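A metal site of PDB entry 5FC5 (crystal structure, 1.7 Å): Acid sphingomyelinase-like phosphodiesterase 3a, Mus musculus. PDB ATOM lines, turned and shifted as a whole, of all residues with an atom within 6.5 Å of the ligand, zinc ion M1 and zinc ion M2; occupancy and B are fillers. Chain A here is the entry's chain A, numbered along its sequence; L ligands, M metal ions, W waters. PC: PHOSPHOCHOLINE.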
ATOM      1  N   ASP A  30      13.848  29.764 -18.341  1.00  0.00           N
ATOM      2  CA  ASP A  30      13.961  30.424 -19.643  1.00  0.00           C
ATOM      3  C   ASP A  30      13.174  31.738 -19.694  1.00  0.00           C
ATOM      4  O   ASP A  30      12.314  31.967 -20.536  1.00  0.00           O
ATOM      5  CB  ASP A  30      13.528  29.444 -20.735  1.00  0.00           C
ATOM      6  CG  ASP A  30      14.523  28.289 -20.881  1.00  0.00           C
ATOM      7  OD1 ASP A  30      14.426  27.287 -20.139  1.00  0.00           O
ATOM      8  OD2 ASP A  30      15.469  28.408 -21.691  1.00  0.00           O
ATOM      9  N   LEU A  31      13.517  32.622 -18.759  1.00  0.00           N
ATOM     10  CA  LEU A  31      12.882  33.928 -18.643  1.00  0.00           C
ATOM     11  C   LEU A  31      13.252  34.824 -19.820  1.00  0.00           C
ATOM     12  O   LEU A  31      12.403  35.540 -20.336  1.00  0.00           O
ATOM     13  CB  LEU A  31      13.290  34.584 -17.323  1.00  0.00           C
ATOM     14  CG  LEU A  31      12.944  33.790 -16.068  1.00  0.00           C
ATOM     15  CD1 LEU A  31      13.583  34.476 -14.863  1.00  0.00           C
ATOM     16  CD2 LEU A  31      11.464  33.656 -15.907  1.00  0.00           C
ATOM     17  N   HIS A  32      14.526  34.781 -20.269  1.00  0.00           N
ATOM     18  CA  HIS A  32      15.015  35.544 -21.423  1.00  0.00           C
ATOM     19  C   HIS A  32      14.475  36.966 -21.434  1.00  0.00           C
ATOM     20  O   HIS A  32      13.694  37.331 -22.318  1.00  0.00           O
ATOM     21  CB  HIS A  32      14.635  34.824 -22.706  1.00  0.00           C
ATOM     22  CG  HIS A  32      15.367  33.535 -22.902  1.00  0.00           C
ATOM     23  ND1 HIS A  32      16.716  33.508 -23.171  1.00  0.00           N
ATOM     24  CD2 HIS A  32      14.945  32.259 -22.893  1.00  0.00           C
ATOM     25  CE1 HIS A  32      17.107  32.248 -23.307  1.00  0.00           C
ATOM     26  NE2 HIS A  32      16.036  31.473 -23.177  1.00  0.00           N
ATOM     27  N   GLY A  94      17.424  28.540 -15.512  1.00  0.00           N
ATOM     28  CA  GLY A  94      18.412  29.285 -16.287  1.00  0.00           C
ATOM     29  C   GLY A  94      17.858  30.012 -17.501  1.00  0.00           C
ATOM     30  O   GLY A  94      16.659  30.032 -17.763  1.00  0.00           O
ATOM     31  N   ASP A  95      18.811  30.609 -18.257  1.00  0.00           N
ATOM     32  CA  ASP A  95      18.626  31.329 -19.520  1.00  0.00           C
ATOM     33  C   ASP A  95      17.909  32.679 -19.355  1.00  0.00           C
ATOM     34  O   ASP A  95      16.735  32.817 -19.767  1.00  0.00           O
ATOM     35  CB  ASP A  95      17.869  30.456 -20.540  1.00  0.00           C
ATOM     36  CG  ASP A  95      18.804  29.826 -21.550  1.00  0.00           C
ATOM     37  OD1 ASP A  95      20.039  29.874 -21.359  1.00  0.00           O
ATOM     38  OD2 ASP A  95      18.301  29.261 -22.550  1.00  0.00           O
ATOM     39  N   HIS A  99      17.864  36.605 -26.718  1.00  0.00           N
ATOM     40  CA  HIS A  99      18.485  36.048 -27.933  1.00  0.00           C
ATOM     41  C   HIS A  99      18.849  37.212 -28.866  1.00  0.00           C
ATOM     42  O   HIS A  99      18.031  37.676 -29.665  1.00  0.00           O
ATOM     43  CB  HIS A  99      17.596  35.048 -28.660  1.00  0.00           C
ATOM     44  CG  HIS A  99      17.195  33.872 -27.832  1.00  0.00           C
ATOM     45  ND1 HIS A  99      16.226  33.947 -26.854  1.00  0.00           N
ATOM     46  CD2 HIS A  99      17.609  32.577 -27.867  1.00  0.00           C
ATOM     47  CE1 HIS A  99      16.073  32.756 -26.296  1.00  0.00           C
ATOM     48  NE2 HIS A  99      16.906  31.906 -26.885  1.00  0.00           N
ATOM     49  N   GLY A 135      21.929  28.525 -17.459  1.00  0.00           N
ATOM     50  CA  GLY A 135      21.603  28.173 -18.836  1.00  0.00           C
ATOM     51  C   GLY A 135      22.710  28.578 -19.794  1.00  0.00           C
ATOM     52  O   GLY A 135      23.659  29.294 -19.449  1.00  0.00           O
ATOM     53  N   ASN A 136      22.570  28.127 -21.046  1.00  0.00           N
ATOM     54  CA  ASN A 136      23.645  28.364 -22.007  1.00  0.00           C
ATOM     55  C   ASN A 136      23.735  29.835 -22.376  1.00  0.00           C
ATOM     56  O   ASN A 136      24.819  30.289 -22.759  1.00  0.00           O
ATOM     57  CB  ASN A 136      23.447  27.466 -23.225  1.00  0.00           C
ATOM     58  CG  ASN A 136      22.073  27.610 -23.846  1.00  0.00           C
ATOM     59  OD1 ASN A 136      21.048  27.277 -23.224  1.00  0.00           O
ATOM     60  ND2 ASN A 136      22.028  28.113 -25.051  1.00  0.00           N
ATOM     61  N   HIS A 137      22.665  30.602 -22.204  1.00  0.00           N
ATOM     62  CA  HIS A 137      22.767  32.017 -22.446  1.00  0.00           C
ATOM     63  C   HIS A 137      23.280  32.796 -21.244  1.00  0.00           C
ATOM     64  O   HIS A 137      23.527  34.000 -21.377  1.00  0.00           O
ATOM     65  CB  HIS A 137      21.403  32.553 -22.872  1.00  0.00           C
ATOM     66  CG  HIS A 137      21.018  32.136 -24.252  1.00  0.00           C
ATOM     67  ND1 HIS A 137      21.362  32.878 -25.366  1.00  0.00           N
ATOM     68  CD2 HIS A 137      20.382  31.035 -24.710  1.00  0.00           C
ATOM     69  CE1 HIS A 137      20.922  32.267 -26.453  1.00  0.00           C
ATOM     70  NE2 HIS A 137      20.306  31.152 -26.090  1.00  0.00           N
ATOM     71  N   GLN A 142      27.605  33.524 -25.486  1.00  0.00           N
ATOM     72  CA  GLN A 142      26.644  32.479 -25.176  1.00  0.00           C
ATOM     73  C   GLN A 142      27.232  31.120 -25.506  1.00  0.00           C
ATOM     74  O   GLN A 142      28.041  30.955 -26.442  1.00  0.00           O
ATOM     75  CB  GLN A 142      25.343  32.685 -25.949  1.00  0.00           C
ATOM     76  CG  GLN A 142      25.422  32.478 -27.458  1.00  0.00           C
ATOM     77  CD  GLN A 142      24.061  32.420 -28.113  1.00  0.00           C
ATOM     78  OE1 GLN A 142      23.420  33.459 -28.336  1.00  0.00           O
ATOM     79  NE2 GLN A 142      23.585  31.203 -28.393  1.00  0.00           N
ATOM     80  N   ASP A 143      26.808  30.142 -24.702  1.00  0.00           N
ATOM     81  CA  ASP A 143      27.132  28.725 -24.823  1.00  0.00           C
ATOM     82  C   ASP A 143      28.575  28.389 -24.458  1.00  0.00           C
ATOM     83  O   ASP A 143      28.913  27.203 -24.362  1.00  0.00           O
ATOM     84  CB  ASP A 143      26.876  28.207 -26.240  1.00  0.00           C
ATOM     85  CG  ASP A 143      25.520  28.591 -26.786  1.00  0.00           C
ATOM     86  OD1 ASP A 143      24.530  28.668 -26.024  1.00  0.00           O
ATOM     87  OD2 ASP A 143      25.443  28.824 -28.026  1.00  0.00           O
ATOM     88  N   ASN A 196      25.304  22.749 -19.568  1.00  0.00           N
ATOM     89  CA  ASN A 196      25.855  23.510 -20.679  1.00  0.00           C
ATOM     90  C   ASN A 196      27.299  23.118 -20.978  1.00  0.00           C
ATOM     91  O   ASN A 196      27.796  23.442 -22.069  1.00  0.00           O
ATOM     92  CB  ASN A 196      25.752  25.001 -20.365  1.00  0.00           C
ATOM     93  CG  ASN A 196      24.406  25.377 -19.848  1.00  0.00           C
ATOM     94  OD1 ASN A 196      23.416  25.376 -20.585  1.00  0.00           O
ATOM     95  ND2 ASN A 196      24.335  25.663 -18.591  1.00  0.00           N
ATOM     96  N   TYR A 199      26.767  20.813 -23.899  1.00  0.00           N
ATOM     97  CA  TYR A 199      25.983  21.322 -25.020  1.00  0.00           C
ATOM     98  C   TYR A 199      26.880  21.541 -26.253  1.00  0.00           C
ATOM     99  O   TYR A 199      27.979  22.082 -26.166  1.00  0.00           O
ATOM    100  CB  TYR A 199      25.273  22.627 -24.564  1.00  0.00           C
ATOM    101  CG  TYR A 199      24.281  23.229 -25.486  1.00  0.00           C
ATOM    102  CD1 TYR A 199      23.324  22.477 -26.147  1.00  0.00           C
ATOM    103  CD2 TYR A 199      24.294  24.608 -25.697  1.00  0.00           C
ATOM    104  CE1 TYR A 199      22.417  23.076 -26.966  1.00  0.00           C
ATOM    105  CE2 TYR A 199      23.389  25.208 -26.530  1.00  0.00           C
ATOM    106  CZ  TYR A 199      22.455  24.446 -27.160  1.00  0.00           C
ATOM    107  OH  TYR A 199      21.568  25.051 -28.005  1.00  0.00           O
ATOM    108  N   HIS A 237      19.792  22.938 -16.958  1.00  0.00           N
ATOM    109  CA  HIS A 237      19.214  23.698 -18.067  1.00  0.00           C
ATOM    110  C   HIS A 237      18.966  22.771 -19.256  1.00  0.00           C
ATOM    111  O   HIS A 237      17.812  22.453 -19.554  1.00  0.00           O
ATOM    112  CB  HIS A 237      20.090  24.899 -18.431  1.00  0.00           C
ATOM    113  CG  HIS A 237      19.500  25.723 -19.511  1.00  0.00           C
ATOM    114  ND1 HIS A 237      18.323  26.451 -19.360  1.00  0.00           N
ATOM    115  CD2 HIS A 237      19.868  25.882 -20.801  1.00  0.00           C
ATOM    116  CE1 HIS A 237      18.016  27.022 -20.500  1.00  0.00           C
ATOM    117  NE2 HIS A 237      18.947  26.721 -21.392  1.00  0.00           N
ATOM    118  N   VAL A 238      20.015  22.345 -19.953  1.00  0.00           N
ATOM    119  CA  VAL A 238      19.864  21.470 -21.122  1.00  0.00           C
ATOM    120  C   VAL A 238      19.548  20.060 -20.613  1.00  0.00           C
ATOM    121  O   VAL A 238      20.229  19.578 -19.703  1.00  0.00           O
ATOM    122  CB  VAL A 238      21.128  21.471 -21.977  1.00  0.00           C
ATOM    123  CG1 VAL A 238      20.903  20.672 -23.273  1.00  0.00           C
ATOM    124  CG2 VAL A 238      21.549  22.893 -22.238  1.00  0.00           C
ATOM    125  N   LEU A 243      16.165  15.221 -28.804  1.00  0.00           N
ATOM    126  CA  LEU A 243      15.232  16.262 -29.232  1.00  0.00           C
ATOM    127  C   LEU A 243      13.943  15.614 -29.750  1.00  0.00           C
ATOM    128  O   LEU A 243      14.006  14.675 -30.533  1.00  0.00           O
ATOM    129  CB  LEU A 243      15.821  17.115 -30.341  1.00  0.00           C
ATOM    130  CG  LEU A 243      17.133  17.839 -30.088  1.00  0.00           C
ATOM    131  CD1 LEU A 243      17.518  18.662 -31.337  1.00  0.00           C
ATOM    132  CD2 LEU A 243      17.001  18.696 -28.903  1.00  0.00           C
ATOM    133  N   TYR A 245      11.648  16.776 -31.682  1.00  0.00           N
ATOM    134  CA  TYR A 245      11.199  17.370 -32.953  1.00  0.00           C
ATOM    135  C   TYR A 245      12.185  17.142 -34.070  1.00  0.00           C
ATOM    136  O   TYR A 245      11.999  17.683 -35.169  1.00  0.00           O
ATOM    137  CB  TYR A 245      11.000  18.892 -32.777  1.00  0.00           C
ATOM    138  CG  TYR A 245      12.231  19.624 -32.291  1.00  0.00           C
ATOM    139  CD1 TYR A 245      12.431  19.816 -30.920  1.00  0.00           C
ATOM    140  CD2 TYR A 245      13.172  20.118 -33.173  1.00  0.00           C
ATOM    141  CE1 TYR A 245      13.565  20.452 -30.442  1.00  0.00           C
ATOM    142  CE2 TYR A 245      14.300  20.778 -32.708  1.00  0.00           C
ATOM    143  CZ  TYR A 245      14.480  20.934 -31.334  1.00  0.00           C
ATOM    144  OH  TYR A 245      15.553  21.560 -30.878  1.00  0.00           O
ATOM    145  N   GLY A 277      15.018  22.649 -18.396  1.00  0.00           N
ATOM    146  CA  GLY A 277      14.462  23.706 -19.220  1.00  0.00           C
ATOM    147  C   GLY A 277      15.045  23.616 -20.622  1.00  0.00           C
ATOM    148  O   GLY A 277      15.087  22.521 -21.193  1.00  0.00           O
ATOM    149  N   HIS A 278      15.453  24.768 -21.166  1.00  0.00           N
ATOM    150  CA  HIS A 278      16.093  24.927 -22.480  1.00  0.00           C
ATOM    151  C   HIS A 278      15.238  24.713 -23.737  1.00  0.00           C
ATOM    152  O   HIS A 278      15.395  25.430 -24.718  1.00  0.00           O
ATOM    153  CB  HIS A 278      17.307  23.993 -22.557  1.00  0.00           C
ATOM    154  CG  HIS A 278      18.086  24.136 -23.827  1.00  0.00           C
ATOM    155  ND1 HIS A 278      18.821  25.263 -24.147  1.00  0.00           N
ATOM    156  CD2 HIS A 278      18.269  23.260 -24.836  1.00  0.00           C
ATOM    157  CE1 HIS A 278      19.400  25.073 -25.318  1.00  0.00           C
ATOM    158  NE2 HIS A 278      19.087  23.869 -25.756  1.00  0.00           N
ATOM    159  N   THR A 279      14.366  23.718 -23.763  1.00  0.00           N
ATOM    160  CA  THR A 279      13.639  23.427 -24.971  1.00  0.00           C
ATOM    161  C   THR A 279      12.494  24.406 -25.206  1.00  0.00           C
ATOM    162  O   THR A 279      12.065  24.552 -26.349  1.00  0.00           O
ATOM    163  CB  THR A 279      13.066  22.018 -24.928  1.00  0.00           C
ATOM    164  OG1 THR A 279      11.959  22.006 -24.040  1.00  0.00           O
ATOM    165  CG2 THR A 279      14.140  21.004 -24.482  1.00  0.00           C
ATOM    166  N   HIS A 280      12.048  25.121 -24.178  1.00  0.00           N
ATOM    167  CA  HIS A 280      10.911  26.042 -24.242  1.00  0.00           C
ATOM    168  C   HIS A 280       9.610  25.318 -24.530  1.00  0.00           C
ATOM    169  O   HIS A 280       8.609  25.939 -24.961  1.00  0.00           O
ATOM    170  CB  HIS A 280      11.162  27.153 -25.262  1.00  0.00           C
ATOM    171  CG  HIS A 280      12.303  28.062 -24.936  1.00  0.00           C
ATOM    172  ND1 HIS A 280      12.409  29.311 -25.504  1.00  0.00           N
ATOM    173  CD2 HIS A 280      13.383  27.924 -24.129  1.00  0.00           C
ATOM    174  CE1 HIS A 280      13.518  29.897 -25.087  1.00  0.00           C
ATOM    175  NE2 HIS A 280      14.132  29.072 -24.233  1.00  0.00           N
ATOM    176  N   ALA A 303       9.040  27.584 -21.343  1.00  0.00           N
ATOM    177  CA  ALA A 303       9.649  28.847 -20.982  1.00  0.00           C
ATOM    178  C   ALA A 303       8.597  29.897 -20.604  1.00  0.00           C
ATOM    179  O   ALA A 303       7.439  29.831 -21.014  1.00  0.00           O
ATOM    180  CB  ALA A 303      10.446  29.377 -22.157  1.00  0.00           C
ATOM    181  N   THR A 305       9.458  33.046 -21.796  1.00  0.00           N
ATOM    182  CA  THR A 305       9.507  33.747 -23.075  1.00  0.00           C
ATOM    183  C   THR A 305       8.671  32.994 -24.100  1.00  0.00           C
ATOM    184  O   THR A 305       8.641  31.751 -24.093  1.00  0.00           O
ATOM    185  CB  THR A 305      10.922  33.928 -23.599  1.00  0.00           C
ATOM    186  OG1 THR A 305      10.860  34.670 -24.833  1.00  0.00           O
ATOM    187  CG2 THR A 305      11.623  32.553 -23.916  1.00  0.00           C
ATOM    188  N   VAL A 307       9.299  33.504 -27.405  1.00  0.00           N
ATOM    189  CA  VAL A 307      10.045  33.821 -28.609  1.00  0.00           C
ATOM    190  C   VAL A 307      10.140  32.643 -29.568  1.00  0.00           C
ATOM    191  O   VAL A 307      10.285  31.473 -29.152  1.00  0.00           O
ATOM    192  CB  VAL A 307      11.444  34.340 -28.239  1.00  0.00           C
ATOM    193  CG1 VAL A 307      12.361  33.170 -27.711  1.00  0.00           C
ATOM    194  CG2 VAL A 307      12.097  35.051 -29.404  1.00  0.00           C
ATOM    195  N   GLN A 312       9.932  29.415 -37.850  1.00  0.00           N
ATOM    196  CA  GLN A 312       9.131  28.456 -37.104  1.00  0.00           C
ATOM    197  C   GLN A 312       7.660  28.753 -37.253  1.00  0.00           C
ATOM    198  O   GLN A 312       7.240  29.904 -37.245  1.00  0.00           O
ATOM    199  CB  GLN A 312       9.492  28.493 -35.606  1.00  0.00           C
ATOM    200  CG  GLN A 312      10.870  28.064 -35.259  1.00  0.00           C
ATOM    201  CD  GLN A 312      11.130  28.301 -33.752  1.00  0.00           C
ATOM    202  OE1 GLN A 312      11.991  29.095 -33.392  1.00  0.00           O
ATOM    203  NE2 GLN A 312      10.299  27.679 -32.890  1.00  0.00           N
HETATM  204  P1   PC L   1      17.986  28.556 -26.012  1.00  0.00           P
HETATM  205  O1   PC L   1      18.594  29.335 -27.186  1.00  0.00           O
HETATM  206  O3   PC L   1      17.041  29.414 -25.337  1.00  0.00           O
HETATM  207  O4   PC L   1      19.202  28.196 -25.197  1.00  0.00           O
HETATM  208  O2   PC L   1      17.341  27.209 -26.644  1.00  0.00           O
HETATM  209  C1   PC L   1      16.026  27.311 -27.102  1.00  0.00           C
HETATM  210  C2   PC L   1      15.653  26.050 -27.927  1.00  0.00           C
HETATM  211  N1   PC L   1      16.249  26.045 -29.261  1.00  0.00           N
HETATM  212  C3   PC L   1      17.722  25.916 -29.241  1.00  0.00           C
HETATM  213  C4   PC L   1      15.849  27.238 -30.019  1.00  0.00           C
HETATM  214  C5   PC L   1      15.691  24.897 -29.961  1.00  0.00           C
HETATM  215 ZN    ZN M   1      16.044  29.395 -23.396  1.00  0.00          ZN
HETATM  216 ZN    ZN M   2      19.026  27.220 -23.352  1.00  0.00          ZN
HETATM  217  O   HOH W   1      17.828  29.978 -30.452  1.00  0.00           O
HETATM  218  O   HOH W   2      19.184  22.970 -28.493  1.00  0.00           O
HETATM  219  O   HOH W   3      16.760  27.467 -24.117  1.00  0.00           O
HETATM  220  O   HOH W   4      15.603  22.138 -27.979  1.00  0.00           O
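Water W3 bridges O of His 278 (2.5 Å) and O2 of the ligand (2.6 Å). Water W2 bridges NE2 of His 278 (2.9 Å) and OH of Tyr 199 (3.2 Å).
Within 4 Å of zinc ion M1: Asp 30, His 32, Asp 95 and His 280. Along chain A the residues within 4 Å of zinc ion M1 span positions 30 to 280.
Zinc ion M2 is bound by a ring nitrogen (NE2) of His 237 (2.0 Å), the side-chain amide oxygen of Asn 136 (2.0 Å), an oxygen (O4) of the ligand (2.1 Å), a ring nitrogen (ND1) of His 278 (2.1 Å), the side-chain carboxylate of Asp 95 (2.3 Å) and water W3 (2.4 Å). Zinc ion M2 has six donor atoms within binding distance.
The side-chain carboxylate (OD2) of Asp 30 is bound to zinc ion M1 (2.1 Å). Zinc ion M1 is bound by a ring nitrogen (NE2) of His 32, at 2.1 Å. NE2 of His 280 is bound to zinc ion M1. Water W3 binds zinc ion M1. O3 of the ligand is bound to zinc ion M1. OD2 of Asp 95 is bound to zinc ion M1, at 2.4 Å.
Of the 25 residues printed, 4 come within 4 Å of zinc ion M2.
The backbone carbonyl oxygen of His 237 lies within hydrogen-bond range of the backbone NH of Gly 277, 3.0 Å away. The side-chain amide nitrogen (ND2) of Asn 136 is in hydrogen-bond range of the side-chain carboxylate (OD1) of Asp 143 (2.7 Å). The backbone NH of Asn 136 sits at hydrogen-bond distance from the side-chain amide oxygen of Asn 196 (2.9 Å). The side-chain carboxylate of Asp 30 sits at hydrogen-bond distance from the backbone NH of His 278 (2.9 Å). The backbone carbonyl oxygen of Asp 30 sits at hydrogen-bond distance from the backbone NH of Thr 305, at 3.3 Å. The backbone carbonyl oxygen (O) of Gly 94 is in hydrogen-bond range of the backbone NH (N) of Asp 30 (2.9 Å). The side-chain carboxylate of Asp 95 is in hydrogen-bond range of the backbone NH of His 137 (2.9 Å). The backbone carbonyl oxygen (O) of Asp 95 is in hydrogen-bond range of the backbone NH (N) of Leu 31, at 3.4 Å.
Tyr 245 touches the ligand. Eight residues have an atom within 4 Å of the ligand: His 32, Asp 95, His 99, Asn 136, His 137, Tyr 245, His 278 and His 280.
O1 of the ligand is in hydrogen-bond range of NE2 of His 137 (2.7 Å). A ring nitrogen (NE2) of His 99 is in hydrogen-bond range of an oxygen (O1) of the ligand (3.1 Å).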
